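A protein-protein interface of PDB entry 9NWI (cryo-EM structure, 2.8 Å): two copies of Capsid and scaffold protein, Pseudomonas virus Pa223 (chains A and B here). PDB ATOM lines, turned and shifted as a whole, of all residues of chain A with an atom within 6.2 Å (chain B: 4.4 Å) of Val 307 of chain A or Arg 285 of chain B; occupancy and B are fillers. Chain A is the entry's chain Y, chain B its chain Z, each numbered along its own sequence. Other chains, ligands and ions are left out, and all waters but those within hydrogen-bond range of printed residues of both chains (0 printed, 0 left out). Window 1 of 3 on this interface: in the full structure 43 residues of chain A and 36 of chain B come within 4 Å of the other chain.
The guanidinium group (NH2) of Arg 285 of chain B lies within hydrogen-bond range of the backbone carbonyl oxygen (O) of His 306 of chain A (3.2 Å). The backbone carbonyl oxygen (O) of Phe 289 of chain B is in hydrogen-bond range of the side-chain amino group (NZ) of Lys 386 of chain A.
The side-chain carboxylate of Asp 267 of chain B lies within salt-bridge range of the guanidinium group of Arg 285 of chain B (3.9 Å). The backbone NH (N) of Asp 281 of chain B lies within hydrogen-bond range of the side-chain hydroxyl (OG) of Ser 278 of chain B, at 3.2 Å. The backbone NH (N) of Arg 285 of chain B is in hydrogen-bond range of the side-chain carboxylate (OD2) of Asp 17 of chain B, at 3.3 Å. The backbone carbonyl oxygen of Gly 266 of chain B is in hydrogen-bond range of the guanidinium group of Arg 285 of chain B (3.0 Å). OD1 of Asp 305 of chain A sits close to N of Val 307 of chain A, 3.4 Å away. NZ of Lys 37 of chain A sits at hydrogen-bond distance from OG1 of Thr 309 of chain A (3.2 Å).
NH2 of Arg 285 of chain B touches O of Val 307 of chain A, 3.7 Å away. CG2 of Thr 309 of chain A touches NH1 of Arg 285 of chain B (3.8 Å). CD of Lys 335 of chain A touches OD2 of Asp 281 of chain B (3.2 Å). N of Gly 266 of chain B touches O of Ala 385 of chain A (3.8 Å).
Val 307 of chain A touches one residue of chain B. Glu 310 of chain A touches none of the printed residues of chain B. Of the printed residues of chain A, Gly 266 of chain B touches Ala 385 (3.8 Å). Of the printed residues of chain A, Asp 281 of chain B touches Lys 335. Arg 285 of chain B touches just these residues of chain A: His 306 (3.2 Å), Val 307 (3.7 Å) and Thr 309 (3.8 Å). Of the printed residues of chain A, Phe 289 of chain B touches Lys 386. The nearest residue of chain A that does not touch Arg 285 of chain B is Lys 335 of chain A (5.3 Å). The nearest printed residue of chain A that does not touch Phe 289 of chain B is Ala 385 of chain A (4.5 Å).
Of the 12 printed residues of chain A, 6 touch a printed residue of chain B. Of the 13 printed residues of chain B, 4 touch a printed residue of chain A. Among the printed residues, no Asp or Glu carboxylate lies within 4 Å of a Lys or Arg side-chain nitrogen of the other chain.
No position is printed for both chains. Of the 6 pairs that touch across the chains among the printed residues, none has its exchanged pair printed and touching as well.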
ATOM      1  N   LYS A  37      -7.965 -12.208  28.119  1.00  0.00           N
ATOM      2  CA  LYS A  37      -7.242 -11.085  27.539  1.00  0.00           C
ATOM      3  C   LYS A  37      -5.908 -10.936  28.247  1.00  0.00           C
ATOM      4  O   LYS A  37      -5.858 -10.938  29.480  1.00  0.00           O
ATOM      5  CB  LYS A  37      -8.054  -9.793  27.654  1.00  0.00           C
ATOM      6  CG  LYS A  37      -7.430  -8.603  26.948  1.00  0.00           C
ATOM      7  CD  LYS A  37      -7.018  -8.954  25.528  1.00  0.00           C
ATOM      8  CE  LYS A  37      -6.268  -7.808  24.873  1.00  0.00           C
ATOM      9  NZ  LYS A  37      -6.065  -8.037  23.417  1.00  0.00           N
ATOM     10  N   ASP A 305     -15.032  -5.919  18.054  1.00  0.00           N
ATOM     11  CA  ASP A 305     -14.540  -5.013  19.088  1.00  0.00           C
ATOM     12  C   ASP A 305     -13.059  -4.790  18.803  1.00  0.00           C
ATOM     13  O   ASP A 305     -12.217  -5.607  19.189  1.00  0.00           O
ATOM     14  CB  ASP A 305     -14.766  -5.594  20.480  1.00  0.00           C
ATOM     15  CG  ASP A 305     -14.494  -4.592  21.586  1.00  0.00           C
ATOM     16  OD1 ASP A 305     -13.854  -3.554  21.319  1.00  0.00           O
ATOM     17  OD2 ASP A 305     -14.915  -4.848  22.733  1.00  0.00           O
ATOM     18  N   HIS A 306     -12.748  -3.687  18.121  1.00  0.00           N
ATOM     19  CA  HIS A 306     -11.371  -3.435  17.710  1.00  0.00           C
ATOM     20  C   HIS A 306     -10.487  -3.088  18.898  1.00  0.00           C
ATOM     21  O   HIS A 306      -9.308  -3.455  18.929  1.00  0.00           O
ATOM     22  CB  HIS A 306     -11.332  -2.321  16.669  1.00  0.00           C
ATOM     23  CG  HIS A 306     -12.140  -2.616  15.446  1.00  0.00           C
ATOM     24  ND1 HIS A 306     -13.400  -2.096  15.244  1.00  0.00           N
ATOM     25  CD2 HIS A 306     -11.872  -3.383  14.364  1.00  0.00           C
ATOM     26  CE1 HIS A 306     -13.871  -2.527  14.088  1.00  0.00           C
ATOM     27  NE2 HIS A 306     -12.963  -3.310  13.535  1.00  0.00           N
ATOM     28  N   VAL A 307     -11.031  -2.369  19.882  1.00  0.00           N
ATOM     29  CA  VAL A 307     -10.238  -1.997  21.049  1.00  0.00           C
ATOM     30  C   VAL A 307      -9.821  -3.238  21.825  1.00  0.00           C
ATOM     31  O   VAL A 307      -8.663  -3.370  22.240  1.00  0.00           O
ATOM     32  CB  VAL A 307     -11.018  -1.011  21.935  1.00  0.00           C
ATOM     33  CG1 VAL A 307     -10.203  -0.652  23.162  1.00  0.00           C
ATOM     34  CG2 VAL A 307     -11.372   0.233  21.146  1.00  0.00           C
ATOM     35  N   ASN A 308     -10.750  -4.167  22.030  1.00  0.00           N
ATOM     36  CA  ASN A 308     -10.451  -5.408  22.726  1.00  0.00           C
ATOM     37  C   ASN A 308      -9.965  -6.508  21.795  1.00  0.00           C
ATOM     38  O   ASN A 308      -9.577  -7.577  22.280  1.00  0.00           O
ATOM     39  CB  ASN A 308     -11.687  -5.896  23.485  1.00  0.00           C
ATOM     40  CG  ASN A 308     -12.108  -4.942  24.580  1.00  0.00           C
ATOM     41  OD1 ASN A 308     -11.303  -4.561  25.428  1.00  0.00           O
ATOM     42  ND2 ASN A 308     -13.374  -4.547  24.567  1.00  0.00           N
ATOM     43  N   THR A 309      -9.973  -6.270  20.486  1.00  0.00           N
ATOM     44  CA  THR A 309      -9.558  -7.250  19.483  1.00  0.00           C
ATOM     45  C   THR A 309     -10.329  -8.557  19.646  1.00  0.00           C
ATOM     46  O   THR A 309      -9.764  -9.621  19.902  1.00  0.00           O
ATOM     47  CB  THR A 309      -8.049  -7.495  19.541  1.00  0.00           C
ATOM     48  OG1 THR A 309      -7.727  -8.226  20.729  1.00  0.00           O
ATOM     49  CG2 THR A 309      -7.296  -6.180  19.545  1.00  0.00           C
ATOM     50  N   GLU A 310     -11.647  -8.462  19.493  1.00  0.00           N
ATOM     51  CA  GLU A 310     -12.513  -9.614  19.681  1.00  0.00           C
ATOM     52  C   GLU A 310     -13.590  -9.641  18.609  1.00  0.00           C
ATOM     53  O   GLU A 310     -13.970  -8.605  18.060  1.00  0.00           O
ATOM     54  CB  GLU A 310     -13.161  -9.601  21.069  1.00  0.00           C
ATOM     55  CG  GLU A 310     -12.313 -10.238  22.149  1.00  0.00           C
ATOM     56  CD  GLU A 310     -12.717  -9.797  23.541  1.00  0.00           C
ATOM     57  OE1 GLU A 310     -13.900  -9.449  23.735  1.00  0.00           O
ATOM     58  OE2 GLU A 310     -11.852  -9.801  24.442  1.00  0.00           O
ATOM     59  N   LYS A 335      -5.895 -12.107  18.540  1.00  0.00           N
ATOM     60  CA  LYS A 335      -4.495 -11.906  18.880  1.00  0.00           C
ATOM     61  C   LYS A 335      -3.928 -13.028  19.732  1.00  0.00           C
ATOM     62  O   LYS A 335      -2.705 -13.138  19.853  1.00  0.00           O
ATOM     63  CB  LYS A 335      -4.308 -10.573  19.609  1.00  0.00           C
ATOM     64  CG  LYS A 335      -4.833  -9.375  18.843  1.00  0.00           C
ATOM     65  CD  LYS A 335      -3.723  -8.401  18.487  1.00  0.00           C
ATOM     66  CE  LYS A 335      -2.607  -9.080  17.714  1.00  0.00           C
ATOM     67  NZ  LYS A 335      -1.828  -8.106  16.904  1.00  0.00           N
ATOM     68  N   TYR A 352     -21.315  -0.863  16.813  1.00  0.00           N
ATOM     69  CA  TYR A 352     -20.069  -0.450  17.444  1.00  0.00           C
ATOM     70  C   TYR A 352     -19.776   0.981  17.022  1.00  0.00           C
ATOM     71  O   TYR A 352     -19.653   1.260  15.826  1.00  0.00           O
ATOM     72  CB  TYR A 352     -18.926  -1.379  17.033  1.00  0.00           C
ATOM     73  CG  TYR A 352     -17.667  -1.237  17.850  1.00  0.00           C
ATOM     74  CD1 TYR A 352     -17.686  -1.416  19.222  1.00  0.00           C
ATOM     75  CD2 TYR A 352     -16.457  -0.942  17.244  1.00  0.00           C
ATOM     76  CE1 TYR A 352     -16.536  -1.295  19.971  1.00  0.00           C
ATOM     77  CE2 TYR A 352     -15.302  -0.820  17.983  1.00  0.00           C
ATOM     78  CZ  TYR A 352     -15.347  -0.998  19.346  1.00  0.00           C
ATOM     79  OH  TYR A 352     -14.200  -0.876  20.090  1.00  0.00           O
ATOM     80  N   ALA A 385     -11.990   8.731  22.719  1.00  0.00           N
ATOM     81  CA  ALA A 385     -10.927   7.991  22.052  1.00  0.00           C
ATOM     82  C   ALA A 385     -11.215   6.501  21.940  1.00  0.00           C
ATOM     83  O   ALA A 385     -10.459   5.793  21.269  1.00  0.00           O
ATOM     84  CB  ALA A 385      -9.602   8.201  22.786  1.00  0.00           C
ATOM     85  N   LYS A 386     -12.277   6.010  22.570  1.00  0.00           N
ATOM     86  CA  LYS A 386     -12.628   4.598  22.525  1.00  0.00           C
ATOM     87  C   LYS A 386     -14.082   4.446  22.113  1.00  0.00           C
ATOM     88  O   LYS A 386     -14.930   5.264  22.478  1.00  0.00           O
ATOM     89  CB  LYS A 386     -12.403   3.920  23.878  1.00  0.00           C
ATOM     90  CG  LYS A 386     -10.950   3.840  24.300  1.00  0.00           C
ATOM     91  CD  LYS A 386     -10.679   2.568  25.083  1.00  0.00           C
ATOM     92  CE  LYS A 386     -11.473   2.533  26.378  1.00  0.00           C
ATOM     93  NZ  LYS A 386     -11.479   3.853  27.065  1.00  0.00           N
ATOM     94  N   SER A 387     -14.364   3.392  21.354  1.00  0.00           N
ATOM     95  CA  SER A 387     -15.716   3.099  20.915  1.00  0.00           C
ATOM     96  C   SER A 387     -16.444   2.268  21.969  1.00  0.00           C
ATOM     97  O   SER A 387     -15.902   1.935  23.024  1.00  0.00           O
ATOM     98  CB  SER A 387     -15.689   2.382  19.569  1.00  0.00           C
ATOM     99  OG  SER A 387     -16.996   2.038  19.154  1.00  0.00           O
ATOM    100  N   ASP B  17       0.181  -3.820  30.725  1.00  0.00           N
ATOM    101  CA  ASP B  17      -0.966  -4.648  30.376  1.00  0.00           C
ATOM    102  C   ASP B  17      -0.890  -6.036  30.997  1.00  0.00           C
ATOM    103  O   ASP B  17      -1.897  -6.545  31.500  1.00  0.00           O
ATOM    104  CB  ASP B  17      -1.085  -4.764  28.856  1.00  0.00           C
ATOM    105  CG  ASP B  17      -1.769  -3.566  28.236  1.00  0.00           C
ATOM    106  OD1 ASP B  17      -2.116  -2.627  28.983  1.00  0.00           O
ATOM    107  OD2 ASP B  17      -1.959  -3.560  27.002  1.00  0.00           O
ATOM    108  N   GLY B 266      -8.001   4.208  18.786  1.00  0.00           N
ATOM    109  CA  GLY B 266      -8.009   2.973  19.538  1.00  0.00           C
ATOM    110  C   GLY B 266      -6.858   2.035  19.260  1.00  0.00           C
ATOM    111  O   GLY B 266      -6.853   0.920  19.793  1.00  0.00           O
ATOM    112  N   ASP B 267      -5.886   2.443  18.448  1.00  0.00           N
ATOM    113  CA  ASP B 267      -4.743   1.590  18.162  1.00  0.00           C
ATOM    114  C   ASP B 267      -3.600   2.435  17.623  1.00  0.00           C
ATOM    115  O   ASP B 267      -3.818   3.491  17.026  1.00  0.00           O
ATOM    116  CB  ASP B 267      -5.102   0.489  17.161  1.00  0.00           C
ATOM    117  CG  ASP B 267      -4.048  -0.594  17.087  1.00  0.00           C
ATOM    118  OD1 ASP B 267      -3.127  -0.587  17.930  1.00  0.00           O
ATOM    119  OD2 ASP B 267      -4.138  -1.454  16.187  1.00  0.00           O
ATOM    120  N   SER B 278       0.165  -4.031  14.812  1.00  0.00           N
ATOM    121  CA  SER B 278       0.127  -3.144  15.963  1.00  0.00           C
ATOM    122  C   SER B 278       1.404  -3.275  16.780  1.00  0.00           C
ATOM    123  O   SER B 278       1.931  -4.375  16.958  1.00  0.00           O
ATOM    124  CB  SER B 278      -1.083  -3.452  16.841  1.00  0.00           C
ATOM    125  OG  SER B 278      -0.834  -3.085  18.185  1.00  0.00           O
ATOM    126  N   ILE B 280       1.641  -1.259  19.861  1.00  0.00           N
ATOM    127  CA  ILE B 280       1.301  -0.903  21.233  1.00  0.00           C
ATOM    128  C   ILE B 280       0.548  -2.009  21.952  1.00  0.00           C
ATOM    129  O   ILE B 280       0.350  -1.915  23.173  1.00  0.00           O
ATOM    130  CB  ILE B 280       0.475   0.399  21.278  1.00  0.00           C
ATOM    131  CG1 ILE B 280       0.651   1.103  22.622  1.00  0.00           C
ATOM    132  CG2 ILE B 280      -0.990   0.107  21.019  1.00  0.00           C
ATOM    133  CD1 ILE B 280       0.406   2.587  22.569  1.00  0.00           C
ATOM    134  N   ASP B 281       0.129  -3.053  21.245  1.00  0.00           N
ATOM    135  CA  ASP B 281      -0.686  -4.088  21.860  1.00  0.00           C
ATOM    136  C   ASP B 281       0.094  -4.832  22.934  1.00  0.00           C
ATOM    137  O   ASP B 281       1.289  -5.101  22.786  1.00  0.00           O
ATOM    138  CB  ASP B 281      -1.182  -5.072  20.804  1.00  0.00           C
ATOM    139  CG  ASP B 281      -2.185  -6.056  21.360  1.00  0.00           C
ATOM    140  OD1 ASP B 281      -3.055  -5.634  22.149  1.00  0.00           O
ATOM    141  OD2 ASP B 281      -2.099  -7.252  21.016  1.00  0.00           O
ATOM    142  N   GLN B 283       1.369  -4.048  25.641  1.00  0.00           N
ATOM    143  CA  GLN B 283       2.395  -3.377  26.429  1.00  0.00           C
ATOM    144  C   GLN B 283       1.849  -2.204  27.230  1.00  0.00           C
ATOM    145  O   GLN B 283       1.917  -2.228  28.463  1.00  0.00           O
ATOM    146  CB  GLN B 283       3.532  -2.918  25.509  1.00  0.00           C
ATOM    147  CG  GLN B 283       4.021  -3.992  24.561  1.00  0.00           C
ATOM    148  CD  GLN B 283       5.464  -3.792  24.154  1.00  0.00           C
ATOM    149  OE1 GLN B 283       6.312  -3.461  24.981  1.00  0.00           O
ATOM    150  NE2 GLN B 283       5.751  -3.994  22.876  1.00  0.00           N
ATOM    151  N   VAL B 284       1.308  -1.174  26.579  1.00  0.00           N
ATOM    152  CA  VAL B 284       0.758  -0.026  27.294  1.00  0.00           C
ATOM    153  C   VAL B 284      -0.582   0.394  26.706  1.00  0.00           C
ATOM    154  O   VAL B 284      -1.004   1.542  26.871  1.00  0.00           O
ATOM    155  CB  VAL B 284       1.742   1.158  27.292  1.00  0.00           C
ATOM    156  CG1 VAL B 284       3.001   0.816  28.067  1.00  0.00           C
ATOM    157  CG2 VAL B 284       2.091   1.550  25.875  1.00  0.00           C
ATOM    158  N   ARG B 285      -1.259  -0.524  26.015  1.00  0.00           N
ATOM    159  CA  ARG B 285      -2.475  -0.154  25.293  1.00  0.00           C
ATOM    160  C   ARG B 285      -3.562   0.329  26.244  1.00  0.00           C
ATOM    161  O   ARG B 285      -4.132   1.412  26.058  1.00  0.00           O
ATOM    162  CB  ARG B 285      -2.973  -1.338  24.469  1.00  0.00           C
ATOM    163  CG  ARG B 285      -4.043  -0.976  23.462  1.00  0.00           C
ATOM    164  CD  ARG B 285      -4.240  -2.087  22.452  1.00  0.00           C
ATOM    165  NE  ARG B 285      -5.305  -1.777  21.507  1.00  0.00           N
ATOM    166  CZ  ARG B 285      -5.502  -2.422  20.367  1.00  0.00           C
ATOM    167  NH1 ARG B 285      -4.726  -3.427  19.999  1.00  0.00           N
ATOM    168  NH2 ARG B 285      -6.504  -2.050  19.577  1.00  0.00           N
ATOM    169  N   LYS B 286      -3.865  -0.466  27.272  1.00  0.00           N
ATOM    170  CA  LYS B 286      -4.913  -0.089  28.213  1.00  0.00           C
ATOM    171  C   LYS B 286      -4.552   1.185  28.959  1.00  0.00           C
ATOM    172  O   LYS B 286      -5.408   2.050  29.179  1.00  0.00           O
ATOM    173  CB  LYS B 286      -5.169  -1.228  29.196  1.00  0.00           C
ATOM    174  CG  LYS B 286      -6.219  -2.218  28.733  1.00  0.00           C
ATOM    175  CD  LYS B 286      -6.788  -3.002  29.903  1.00  0.00           C
ATOM    176  CE  LYS B 286      -7.126  -2.089  31.069  1.00  0.00           C
ATOM    177  NZ  LYS B 286      -8.316  -2.573  31.821  1.00  0.00           N
ATOM    178  N   PHE B 287      -3.290   1.315  29.367  1.00  0.00           N
ATOM    179  CA  PHE B 287      -2.862   2.525  30.057  1.00  0.00           C
ATOM    180  C   PHE B 287      -2.985   3.745  29.158  1.00  0.00           C
ATOM    181  O   PHE B 287      -3.445   4.804  29.598  1.00  0.00           O
ATOM    182  CB  PHE B 287      -1.424   2.368  30.547  1.00  0.00           C
ATOM    183  CG  PHE B 287      -0.749   3.668  30.864  1.00  0.00           C
ATOM    184  CD1 PHE B 287      -1.036   4.342  32.035  1.00  0.00           C
ATOM    185  CD2 PHE B 287       0.173   4.216  29.992  1.00  0.00           C
ATOM    186  CE1 PHE B 287      -0.418   5.536  32.331  1.00  0.00           C
ATOM    187  CE2 PHE B 287       0.793   5.411  30.282  1.00  0.00           C
ATOM    188  CZ  PHE B 287       0.497   6.071  31.453  1.00  0.00           C
ATOM    189  N   PHE B 288      -2.579   3.619  27.894  1.00  0.00           N
ATOM    190  CA  PHE B 288      -2.599   4.773  27.003  1.00  0.00           C
ATOM    191  C   PHE B 288      -4.023   5.195  26.673  1.00  0.00           C
ATOM    192  O   PHE B 288      -4.367   6.377  26.779  1.00  0.00           O
ATOM    193  CB  PHE B 288      -1.825   4.474  25.723  1.00  0.00           C
ATOM    194  CG  PHE B 288      -1.852   5.599  24.734  1.00  0.00           C
ATOM    195  CD1 PHE B 288      -1.503   6.880  25.114  1.00  0.00           C
ATOM    196  CD2 PHE B 288      -2.242   5.379  23.426  1.00  0.00           C
ATOM    197  CE1 PHE B 288      -1.531   7.917  24.209  1.00  0.00           C
ATOM    198  CE2 PHE B 288      -2.272   6.413  22.517  1.00  0.00           C
ATOM    199  CZ  PHE B 288      -1.916   7.684  22.909  1.00  0.00           C
ATOM    200  N   PHE B 289      -4.872   4.251  26.277  1.00  0.00           N
ATOM    201  CA  PHE B 289      -6.239   4.629  25.919  1.00  0.00           C
ATOM    202  C   PHE B 289      -7.158   4.600  27.135  1.00  0.00           C
ATOM    203  O   PHE B 289      -8.272   4.083  27.104  1.00  0.00           O
ATOM    204  CB  PHE B 289      -6.759   3.717  24.816  1.00  0.00           C
ATOM    205  CG  PHE B 289      -6.128   3.968  23.482  1.00  0.00           C
ATOM    206  CD1 PHE B 289      -6.276   5.190  22.853  1.00  0.00           C
ATOM    207  CD2 PHE B 289      -5.383   2.986  22.860  1.00  0.00           C
ATOM    208  CE1 PHE B 289      -5.694   5.425  21.625  1.00  0.00           C
ATOM    209  CE2 PHE B 289      -4.800   3.216  21.634  1.00  0.00           C
ATOM    210  CZ  PHE B 289      -4.956   4.436  21.015  1.00  0.00           C
